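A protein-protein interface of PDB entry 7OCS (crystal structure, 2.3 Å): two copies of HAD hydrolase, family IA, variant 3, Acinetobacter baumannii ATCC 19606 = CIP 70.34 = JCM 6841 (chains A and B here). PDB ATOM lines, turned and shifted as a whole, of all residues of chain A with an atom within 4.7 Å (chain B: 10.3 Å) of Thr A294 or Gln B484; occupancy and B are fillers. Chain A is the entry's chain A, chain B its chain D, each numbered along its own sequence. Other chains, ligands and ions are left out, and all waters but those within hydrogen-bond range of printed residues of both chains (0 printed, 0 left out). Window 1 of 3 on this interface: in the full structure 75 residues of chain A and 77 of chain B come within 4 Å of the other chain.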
ATOM      1  N   VAL A 289     -32.045 -29.606  -4.535  1.00  0.00           N
ATOM      2  CA  VAL A 289     -31.147 -29.350  -5.659  1.00  0.00           C
ATOM      3  C   VAL A 289     -31.676 -28.235  -6.520  1.00  0.00           C
ATOM      4  O   VAL A 289     -30.911 -27.374  -6.924  1.00  0.00           O
ATOM      5  CB  VAL A 289     -30.851 -30.619  -6.513  1.00  0.00           C
ATOM      6  CG1 VAL A 289     -29.911 -30.290  -7.667  1.00  0.00           C
ATOM      7  CG2 VAL A 289     -30.276 -31.726  -5.660  1.00  0.00           C
ATOM      8  N   PHE A 292     -31.017 -24.740  -5.038  1.00  0.00           N
ATOM      9  CA  PHE A 292     -29.609 -24.333  -5.156  1.00  0.00           C
ATOM     10  C   PHE A 292     -29.112 -24.256  -6.602  1.00  0.00           C
ATOM     11  O   PHE A 292     -28.137 -23.565  -6.886  1.00  0.00           O
ATOM     12  CB  PHE A 292     -28.716 -25.322  -4.382  1.00  0.00           C
ATOM     13  CG  PHE A 292     -28.621 -25.080  -2.897  1.00  0.00           C
ATOM     14  CD1 PHE A 292     -29.689 -25.363  -2.060  1.00  0.00           C
ATOM     15  CD2 PHE A 292     -27.439 -24.639  -2.326  1.00  0.00           C
ATOM     16  CE1 PHE A 292     -29.587 -25.176  -0.688  1.00  0.00           C
ATOM     17  CE2 PHE A 292     -27.339 -24.454  -0.951  1.00  0.00           C
ATOM     18  CZ  PHE A 292     -28.417 -24.713  -0.144  1.00  0.00           C
ATOM     19  N   GLY A 293     -29.727 -25.019  -7.486  1.00  0.00           N
ATOM     20  CA  GLY A 293     -29.282 -25.127  -8.867  1.00  0.00           C
ATOM     21  C   GLY A 293     -28.132 -26.115  -9.038  1.00  0.00           C
ATOM     22  O   GLY A 293     -27.825 -26.537 -10.163  1.00  0.00           O
ATOM     23  N   THR A 294     -27.451 -26.468  -7.901  1.00  0.00           N
ATOM     24  CA  THR A 294     -26.321 -27.393  -7.848  1.00  0.00           C
ATOM     25  C   THR A 294     -26.381 -28.240  -6.532  1.00  0.00           C
ATOM     26  O   THR A 294     -27.117 -27.909  -5.602  1.00  0.00           O
ATOM     27  CB  THR A 294     -24.936 -26.584  -7.856  1.00  0.00           C
ATOM     28  OG1 THR A 294     -24.659 -26.085  -6.539  1.00  0.00           O
ATOM     29  CG2 THR A 294     -24.909 -25.456  -8.839  1.00  0.00           C
ATOM     30  N   TYR A 295     -25.545 -29.276  -6.451  1.00  0.00           N
ATOM     31  CA  TYR A 295     -25.277 -30.022  -5.234  1.00  0.00           C
ATOM     32  C   TYR A 295     -23.758 -30.351  -5.208  1.00  0.00           C
ATOM     33  O   TYR A 295     -23.050 -30.082  -6.189  1.00  0.00           O
ATOM     34  CB  TYR A 295     -26.154 -31.277  -5.110  1.00  0.00           C
ATOM     35  CG  TYR A 295     -25.793 -32.354  -6.096  1.00  0.00           C
ATOM     36  CD1 TYR A 295     -26.355 -32.381  -7.362  1.00  0.00           C
ATOM     37  CD2 TYR A 295     -24.905 -33.360  -5.759  1.00  0.00           C
ATOM     38  CE1 TYR A 295     -26.017 -33.359  -8.275  1.00  0.00           C
ATOM     39  CE2 TYR A 295     -24.549 -34.334  -6.669  1.00  0.00           C
ATOM     40  CZ  TYR A 295     -25.119 -34.338  -7.925  1.00  0.00           C
ATOM     41  OH  TYR A 295     -24.819 -35.318  -8.809  1.00  0.00           O
ATOM     42  N   ARG A 307     -18.455 -29.492  -6.681  1.00  0.00           N
ATOM     43  CA  ARG A 307     -19.752 -28.945  -7.063  1.00  0.00           C
ATOM     44  C   ARG A 307     -20.237 -29.396  -8.456  1.00  0.00           C
ATOM     45  O   ARG A 307     -19.559 -29.170  -9.459  1.00  0.00           O
ATOM     46  CB  ARG A 307     -19.769 -27.424  -6.940  1.00  0.00           C
ATOM     47  CG  ARG A 307     -21.179 -26.855  -6.918  1.00  0.00           C
ATOM     48  CD  ARG A 307     -21.195 -25.356  -6.673  1.00  0.00           C
ATOM     49  NE  ARG A 307     -20.627 -25.014  -5.367  1.00  0.00           N
ATOM     50  CZ  ARG A 307     -20.554 -23.775  -4.884  1.00  0.00           C
ATOM     51  NH1 ARG A 307     -20.019 -23.553  -3.689  1.00  0.00           N
ATOM     52  NH2 ARG A 307     -21.017 -22.751  -5.591  1.00  0.00           N
ATOM     53  N   ILE A 308     -21.416 -30.033  -8.507  1.00  0.00           N
ATOM     54  CA  ILE A 308     -22.009 -30.488  -9.752  1.00  0.00           C
ATOM     55  C   ILE A 308     -22.995 -29.453 -10.220  1.00  0.00           C
ATOM     56  O   ILE A 308     -24.116 -29.374  -9.708  1.00  0.00           O
ATOM     57  CB  ILE A 308     -22.668 -31.882  -9.612  1.00  0.00           C
ATOM     58  CG1 ILE A 308     -21.719 -32.886  -8.933  1.00  0.00           C
ATOM     59  CG2 ILE A 308     -23.157 -32.387 -10.969  1.00  0.00           C
ATOM     60  CD1 ILE A 308     -20.413 -33.178  -9.751  1.00  0.00           C
ATOM     61  N   GLU A 309     -22.577 -28.646 -11.194  1.00  0.00           N
ATOM     62  CA  GLU A 309     -23.361 -27.565 -11.740  1.00  0.00           C
ATOM     63  C   GLU A 309     -24.352 -28.030 -12.828  1.00  0.00           C
ATOM     64  O   GLU A 309     -24.243 -29.147 -13.341  1.00  0.00           O
ATOM     65  CB  GLU A 309     -22.410 -26.489 -12.309  1.00  0.00           C
ATOM     66  CG  GLU A 309     -21.564 -25.824 -11.242  1.00  0.00           C
ATOM     67  CD  GLU A 309     -20.642 -24.735 -11.754  1.00  0.00           C
ATOM     68  OE1 GLU A 309     -20.216 -24.812 -12.930  1.00  0.00           O
ATOM     69  OE2 GLU A 309     -20.349 -23.798 -10.975  1.00  0.00           O
ATOM     70  N   ASN A 310     -25.316 -27.156 -13.163  1.00  0.00           N
ATOM     71  CA  ASN A 310     -26.289 -27.363 -14.231  1.00  0.00           C
ATOM     72  C   ASN A 310     -27.127 -28.611 -14.023  1.00  0.00           C
ATOM     73  O   ASN A 310     -27.402 -29.348 -14.976  1.00  0.00           O
ATOM     74  CB  ASN A 310     -25.588 -27.358 -15.594  1.00  0.00           C
ATOM     75  CG  ASN A 310     -24.708 -26.141 -15.768  1.00  0.00           C
ATOM     76  OD1 ASN A 310     -25.139 -25.007 -15.568  1.00  0.00           O
ATOM     77  ND2 ASN A 310     -23.447 -26.353 -16.082  1.00  0.00           N
ATOM     78  N   LEU A 488     -24.466 -27.665  -1.169  1.00  0.00           N
ATOM     79  CA  LEU A 488     -25.515 -28.571  -0.774  1.00  0.00           C
ATOM     80  C   LEU A 488     -24.930 -29.982  -0.825  1.00  0.00           C
ATOM     81  O   LEU A 488     -24.960 -30.631  -1.867  1.00  0.00           O
ATOM     82  CB  LEU A 488     -26.730 -28.462  -1.697  1.00  0.00           C
ATOM     83  CG  LEU A 488     -27.908 -29.378  -1.328  1.00  0.00           C
ATOM     84  CD1 LEU A 488     -28.503 -29.000   0.025  1.00  0.00           C
ATOM     85  CD2 LEU A 488     -28.958 -29.372  -2.401  1.00  0.00           C
ATOM     86  N   PHE B 292     -23.027  -8.456  -8.701  1.00  0.00           N
ATOM     87  CA  PHE B 292     -22.738  -9.847  -9.071  1.00  0.00           C
ATOM     88  C   PHE B 292     -22.217 -10.685  -7.912  1.00  0.00           C
ATOM     89  O   PHE B 292     -22.422 -11.892  -7.890  1.00  0.00           O
ATOM     90  CB  PHE B 292     -21.710  -9.882 -10.207  1.00  0.00           C
ATOM     91  CG  PHE B 292     -22.279  -9.859 -11.603  1.00  0.00           C
ATOM     92  CD1 PHE B 292     -22.735  -8.679 -12.163  1.00  0.00           C
ATOM     93  CD2 PHE B 292     -22.262 -10.998 -12.394  1.00  0.00           C
ATOM     94  CE1 PHE B 292     -23.212  -8.649 -13.472  1.00  0.00           C
ATOM     95  CE2 PHE B 292     -22.750 -10.968 -13.695  1.00  0.00           C
ATOM     96  CZ  PHE B 292     -23.224  -9.797 -14.225  1.00  0.00           C
ATOM     97  N   THR B 294     -19.136 -11.302  -7.501  1.00  0.00           N
ATOM     98  CA  THR B 294     -17.822 -11.649  -8.022  1.00  0.00           C
ATOM     99  C   THR B 294     -17.546 -10.858  -9.349  1.00  0.00           C
ATOM    100  O   THR B 294     -18.437 -10.205  -9.890  1.00  0.00           O
ATOM    101  CB  THR B 294     -17.793 -13.188  -8.348  1.00  0.00           C
ATOM    102  OG1 THR B 294     -18.698 -13.448  -9.425  1.00  0.00           O
ATOM    103  CG2 THR B 294     -18.139 -14.042  -7.176  1.00  0.00           C
ATOM    104  N   SER B 296     -14.644 -11.537 -13.040  1.00  0.00           N
ATOM    105  CA  SER B 296     -13.713 -12.494 -13.628  1.00  0.00           C
ATOM    106  C   SER B 296     -12.566 -11.847 -14.378  1.00  0.00           C
ATOM    107  O   SER B 296     -12.720 -10.767 -14.951  1.00  0.00           O
ATOM    108  CB  SER B 296     -14.449 -13.479 -14.524  1.00  0.00           C
ATOM    109  OG  SER B 296     -15.347 -14.259 -13.753  1.00  0.00           O
ATOM    110  N   ASP B 305     -11.797 -17.889 -18.111  1.00  0.00           N
ATOM    111  CA  ASP B 305     -12.348 -16.845 -17.244  1.00  0.00           C
ATOM    112  C   ASP B 305     -12.158 -17.247 -15.789  1.00  0.00           C
ATOM    113  O   ASP B 305     -12.742 -18.221 -15.341  1.00  0.00           O
ATOM    114  CB  ASP B 305     -13.836 -16.630 -17.547  1.00  0.00           C
ATOM    115  CG  ASP B 305     -14.084 -16.022 -18.912  1.00  0.00           C
ATOM    116  OD1 ASP B 305     -13.191 -15.298 -19.409  1.00  0.00           O
ATOM    117  OD2 ASP B 305     -15.181 -16.254 -19.478  1.00  0.00           O
ATOM    118  N   ARG B 307     -12.824 -16.678 -12.075  1.00  0.00           N
ATOM    119  CA  ARG B 307     -13.727 -15.981 -11.171  1.00  0.00           C
ATOM    120  C   ARG B 307     -13.077 -15.669  -9.820  1.00  0.00           C
ATOM    121  O   ARG B 307     -12.531 -16.558  -9.171  1.00  0.00           O
ATOM    122  CB  ARG B 307     -15.016 -16.778 -10.979  1.00  0.00           C
ATOM    123  CG  ARG B 307     -16.167 -15.938 -10.418  1.00  0.00           C
ATOM    124  CD  ARG B 307     -17.376 -16.782 -10.069  1.00  0.00           C
ATOM    125  NE  ARG B 307     -17.829 -17.588 -11.204  1.00  0.00           N
ATOM    126  CZ  ARG B 307     -18.830 -17.251 -12.012  1.00  0.00           C
ATOM    127  NH1 ARG B 307     -19.172 -18.041 -13.022  1.00  0.00           N
ATOM    128  NH2 ARG B 307     -19.510 -16.123 -11.806  1.00  0.00           N
ATOM    129  N   GLU B 309     -13.795 -14.623  -6.118  1.00  0.00           N
ATOM    130  CA  GLU B 309     -14.874 -14.605  -5.148  1.00  0.00           C
ATOM    131  C   GLU B 309     -14.548 -13.753  -3.900  1.00  0.00           C
ATOM    132  O   GLU B 309     -13.390 -13.366  -3.685  1.00  0.00           O
ATOM    133  CB  GLU B 309     -15.241 -16.049  -4.739  1.00  0.00           C
ATOM    134  CG  GLU B 309     -16.056 -16.784  -5.788  1.00  0.00           C
ATOM    135  CD  GLU B 309     -16.206 -18.277  -5.566  1.00  0.00           C
ATOM    136  OE1 GLU B 309     -15.526 -18.820  -4.664  1.00  0.00           O
ATOM    137  OE2 GLU B 309     -16.997 -18.908  -6.304  1.00  0.00           O
ATOM    138  N   HIS B 440     -34.289 -15.167 -18.200  1.00  0.00           N
ATOM    139  CA  HIS B 440     -34.222 -16.249 -17.210  1.00  0.00           C
ATOM    140  C   HIS B 440     -35.379 -16.127 -16.201  1.00  0.00           C
ATOM    141  O   HIS B 440     -35.953 -17.138 -15.803  1.00  0.00           O
ATOM    142  CB  HIS B 440     -32.839 -16.230 -16.495  1.00  0.00           C
ATOM    143  CG  HIS B 440     -32.767 -17.035 -15.224  1.00  0.00           C
ATOM    144  ND1 HIS B 440     -33.098 -18.383 -15.197  1.00  0.00           N
ATOM    145  CD2 HIS B 440     -32.359 -16.662 -13.985  1.00  0.00           C
ATOM    146  CE1 HIS B 440     -32.908 -18.774 -13.947  1.00  0.00           C
ATOM    147  NE2 HIS B 440     -32.459 -17.775 -13.182  1.00  0.00           N
ATOM    148  N   MET B 473     -35.362 -20.784   0.026  1.00  0.00           N
ATOM    149  CA  MET B 473     -34.124 -20.919  -0.714  1.00  0.00           C
ATOM    150  C   MET B 473     -34.356 -20.819  -2.216  1.00  0.00           C
ATOM    151  O   MET B 473     -33.601 -20.154  -2.888  1.00  0.00           O
ATOM    152  CB  MET B 473     -33.420 -22.232  -0.348  1.00  0.00           C
ATOM    153  CG  MET B 473     -32.684 -22.152   0.963  1.00  0.00           C
ATOM    154  SD  MET B 473     -32.263 -23.765   1.654  1.00  0.00           S
ATOM    155  CE  MET B 473     -30.916 -23.326   2.619  1.00  0.00           C
ATOM    156  N   PHE B 477     -32.504 -17.958  -4.331  1.00  0.00           N
ATOM    157  CA  PHE B 477     -31.379 -18.396  -5.154  1.00  0.00           C
ATOM    158  C   PHE B 477     -31.702 -18.518  -6.645  1.00  0.00           C
ATOM    159  O   PHE B 477     -30.829 -18.259  -7.463  1.00  0.00           O
ATOM    160  CB  PHE B 477     -30.787 -19.720  -4.634  1.00  0.00           C
ATOM    161  CG  PHE B 477     -30.299 -19.711  -3.197  1.00  0.00           C
ATOM    162  CD1 PHE B 477     -29.773 -18.561  -2.633  1.00  0.00           C
ATOM    163  CD2 PHE B 477     -30.329 -20.866  -2.429  1.00  0.00           C
ATOM    164  CE1 PHE B 477     -29.310 -18.561  -1.328  1.00  0.00           C
ATOM    165  CE2 PHE B 477     -29.868 -20.863  -1.122  1.00  0.00           C
ATOM    166  CZ  PHE B 477     -29.354 -19.715  -0.579  1.00  0.00           C
ATOM    167  N   GLN B 478     -32.938 -18.928  -7.002  1.00  0.00           N
ATOM    168  CA  GLN B 478     -33.328 -19.158  -8.408  1.00  0.00           C
ATOM    169  C   GLN B 478     -32.858 -18.058  -9.417  1.00  0.00           C
ATOM    170  O   GLN B 478     -32.266 -18.411 -10.441  1.00  0.00           O
ATOM    171  CB  GLN B 478     -34.825 -19.411  -8.539  1.00  0.00           C
ATOM    172  CG  GLN B 478     -35.208 -20.119  -9.826  1.00  0.00           C
ATOM    173  CD  GLN B 478     -36.549 -20.811  -9.687  1.00  0.00           C
ATOM    174  OE1 GLN B 478     -36.677 -22.022  -9.922  1.00  0.00           O
ATOM    175  NE2 GLN B 478     -37.582 -20.056  -9.280  1.00  0.00           N
ATOM    176  N   PRO B 479     -33.061 -16.735  -9.156  1.00  0.00           N
ATOM    177  CA  PRO B 479     -32.575 -15.723 -10.119  1.00  0.00           C
ATOM    178  C   PRO B 479     -31.051 -15.763 -10.340  1.00  0.00           C
ATOM    179  O   PRO B 479     -30.575 -15.462 -11.431  1.00  0.00           O
ATOM    180  CB  PRO B 479     -33.003 -14.403  -9.484  1.00  0.00           C
ATOM    181  CG  PRO B 479     -34.136 -14.763  -8.577  1.00  0.00           C
ATOM    182  CD  PRO B 479     -33.762 -16.094  -8.022  1.00  0.00           C
ATOM    183  N   GLY B 480     -30.310 -16.145  -9.308  1.00  0.00           N
ATOM    184  CA  GLY B 480     -28.857 -16.225  -9.372  1.00  0.00           C
ATOM    185  C   GLY B 480     -28.304 -17.519  -9.940  1.00  0.00           C
ATOM    186  O   GLY B 480     -27.088 -17.672 -10.036  1.00  0.00           O
ATOM    187  N   HIS B 481     -29.186 -18.469 -10.334  1.00  0.00           N
ATOM    188  CA  HIS B 481     -28.743 -19.745 -10.928  1.00  0.00           C
ATOM    189  C   HIS B 481     -27.977 -19.528 -12.231  1.00  0.00           C
ATOM    190  O   HIS B 481     -27.082 -20.304 -12.556  1.00  0.00           O
ATOM    191  CB  HIS B 481     -29.931 -20.684 -11.181  1.00  0.00           C
ATOM    192  CG  HIS B 481     -30.520 -21.295  -9.942  1.00  0.00           C
ATOM    193  ND1 HIS B 481     -31.628 -22.113 -10.009  1.00  0.00           N
ATOM    194  CD2 HIS B 481     -30.140 -21.183  -8.645  1.00  0.00           C
ATOM    195  CE1 HIS B 481     -31.889 -22.465  -8.762  1.00  0.00           C
ATOM    196  NE2 HIS B 481     -31.024 -21.924  -7.909  1.00  0.00           N
ATOM    197  N   ILE B 482     -28.322 -18.476 -12.970  1.00  0.00           N
ATOM    198  CA  ILE B 482     -27.664 -18.133 -14.222  1.00  0.00           C
ATOM    199  C   ILE B 482     -26.149 -17.764 -14.008  1.00  0.00           C
ATOM    200  O   ILE B 482     -25.353 -17.901 -14.929  1.00  0.00           O
ATOM    201  CB  ILE B 482     -28.479 -17.013 -14.937  1.00  0.00           C
ATOM    202  CG1 ILE B 482     -28.094 -16.877 -16.409  1.00  0.00           C
ATOM    203  CG2 ILE B 482     -28.388 -15.681 -14.190  1.00  0.00           C
ATOM    204  CD1 ILE B 482     -29.029 -15.945 -17.216  1.00  0.00           C
ATOM    205  N   LEU B 483     -25.758 -17.400 -12.763  1.00  0.00           N
ATOM    206  CA  LEU B 483     -24.370 -17.056 -12.430  1.00  0.00           C
ATOM    207  C   LEU B 483     -23.390 -18.241 -12.483  1.00  0.00           C
ATOM    208  O   LEU B 483     -22.191 -18.036 -12.304  1.00  0.00           O
ATOM    209  CB  LEU B 483     -24.289 -16.369 -11.061  1.00  0.00           C
ATOM    210  CG  LEU B 483     -25.017 -15.034 -10.940  1.00  0.00           C
ATOM    211  CD1 LEU B 483     -24.887 -14.472  -9.534  1.00  0.00           C
ATOM    212  CD2 LEU B 483     -24.495 -14.018 -11.975  1.00  0.00           C
ATOM    213  N   GLN B 484     -23.888 -19.469 -12.707  1.00  0.00           N
ATOM    214  CA  GLN B 484     -23.022 -20.643 -12.825  1.00  0.00           C
ATOM    215  C   GLN B 484     -22.194 -20.560 -14.115  1.00  0.00           C
ATOM    216  O   GLN B 484     -21.026 -20.947 -14.127  1.00  0.00           O
ATOM    217  CB  GLN B 484     -23.852 -21.936 -12.819  1.00  0.00           C
ATOM    218  CG  GLN B 484     -24.475 -22.258 -11.469  1.00  0.00           C
ATOM    219  CD  GLN B 484     -25.450 -23.405 -11.581  1.00  0.00           C
ATOM    220  OE1 GLN B 484     -25.139 -24.467 -12.136  1.00  0.00           O
ATOM    221  NE2 GLN B 484     -26.651 -23.220 -11.047  1.00  0.00           N
ATOM    222  N   SER B 485     -22.801 -20.061 -15.196  1.00  0.00           N
ATOM    223  CA  SER B 485     -22.115 -19.910 -16.472  1.00  0.00           C
ATOM    224  C   SER B 485     -22.137 -18.438 -16.962  1.00  0.00           C
ATOM    225  O   SER B 485     -22.078 -18.189 -18.162  1.00  0.00           O
ATOM    226  CB  SER B 485     -22.737 -20.827 -17.517  1.00  0.00           C
ATOM    227  OG  SER B 485     -24.138 -20.619 -17.591  1.00  0.00           O
ATOM    228  N   MET B 486     -22.222 -17.477 -16.031  1.00  0.00           N
ATOM    229  CA  MET B 486     -22.219 -16.062 -16.367  1.00  0.00           C
ATOM    230  C   MET B 486     -21.177 -15.341 -15.536  1.00  0.00           C
ATOM    231  O   MET B 486     -21.290 -15.281 -14.310  1.00  0.00           O
ATOM    232  CB  MET B 486     -23.602 -15.435 -16.153  1.00  0.00           C
ATOM    233  CG  MET B 486     -23.629 -13.931 -16.414  1.00  0.00           C
ATOM    234  SD  MET B 486     -25.286 -13.241 -16.308  1.00  0.00           S
ATOM    235  CE  MET B 486     -25.978 -13.949 -17.684  1.00  0.00           C
ATOM    236  N   ASP B 487     -20.160 -14.801 -16.193  1.00  0.00           N
ATOM    237  CA  ASP B 487     -19.086 -14.102 -15.515  1.00  0.00           C
ATOM    238  C   ASP B 487     -19.137 -12.596 -15.796  1.00  0.00           C
ATOM    239  O   ASP B 487     -19.529 -12.183 -16.890  1.00  0.00           O
ATOM    240  CB  ASP B 487     -17.725 -14.665 -15.975  1.00  0.00           C
ATOM    241  CG  ASP B 487     -17.467 -16.116 -15.577  1.00  0.00           C
ATOM    242  OD1 ASP B 487     -18.175 -17.013 -16.098  1.00  0.00           O
ATOM    243  OD2 ASP B 487     -16.536 -16.356 -14.776  1.00  0.00           O
ATOM    244  N   LEU B 488     -18.718 -11.775 -14.821  1.00  0.00           N
ATOM    245  CA  LEU B 488     -18.630 -10.338 -15.027  1.00  0.00           C
ATOM    246  C   LEU B 488     -17.183 -10.012 -15.387  1.00  0.00           C
ATOM    247  O   LEU B 488     -16.360  -9.786 -14.502  1.00  0.00           O
ATOM    248  CB  LEU B 488     -19.055  -9.572 -13.771  1.00  0.00           C
ATOM    249  CG  LEU B 488     -18.955  -8.052 -13.870  1.00  0.00           C
ATOM    250  CD1 LEU B 488     -19.882  -7.509 -14.938  1.00  0.00           C
ATOM    251  CD2 LEU B 488     -19.221  -7.406 -12.541  1.00  0.00           C
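O of His B481 lies within hydrogen-bond range of NE2 of Gln B484 (3.3 Å).
Among the printed residues, pairs that only touch across the chains: Glu A309 with Gln B484 (3.4 Å), Thr A294 with Gln B484 (3.4 Å), Gly A293 with Gln B484 (3.6 Å) and Phe A292 with Met B473 (3.8 Å).
No residue of chain B comes within 4 Å of Val A289. Printed residues of chain B within 4 Å of Phe A292: Met B473 (3.8 Å) and His B481 (3.3 Å). Of chain B, only His B481 (3.4 Å) and Gln B484 (3.6 Å) come within 4 Å of Gly A293. Glu A309 touches one residue of chain B. Of chain B, only Gln B484 (2.9 Å) comes within 4 Å of Asn A310. Of the printed residues of chain A, His B481 touches Phe A292 (3.3 Å) and Gly A293 (3.4 Å). Gln B484 touches just these residues of chain A: Gly A293 (3.6 Å), Thr A294 (3.4 Å), Glu A309 (3.4 Å) and Asn A310 (2.9 Å). The nearest residue of chain B that does not touch Thr A294 is His B481 (5.8 Å). The nearest printed residue of chain A that does not touch Met B473 is Leu A488 (6.6 Å).
Of the 20 printed residues of chain B, 3 touch a printed residue of chain A. Among the printed residues, no Asp or Glu carboxylate lies within 4 Å of a Lys or Arg side-chain nitrogen of the other chain.
The backbone NH of Asn A310 lies within hydrogen-bond range of the side-chain amide oxygen of Gln B484. The backbone carbonyl oxygen (O) of Phe A292 sits close to a ring nitrogen (NE2) of His B481 (3.5 Å). A ring nitrogen (NE2) of His B481 lies within hydrogen-bond range of the backbone NH (N) of Gly A293, 3.4 Å away.
Positions printed for both chains: 292, 294, 307, 309 and 488.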
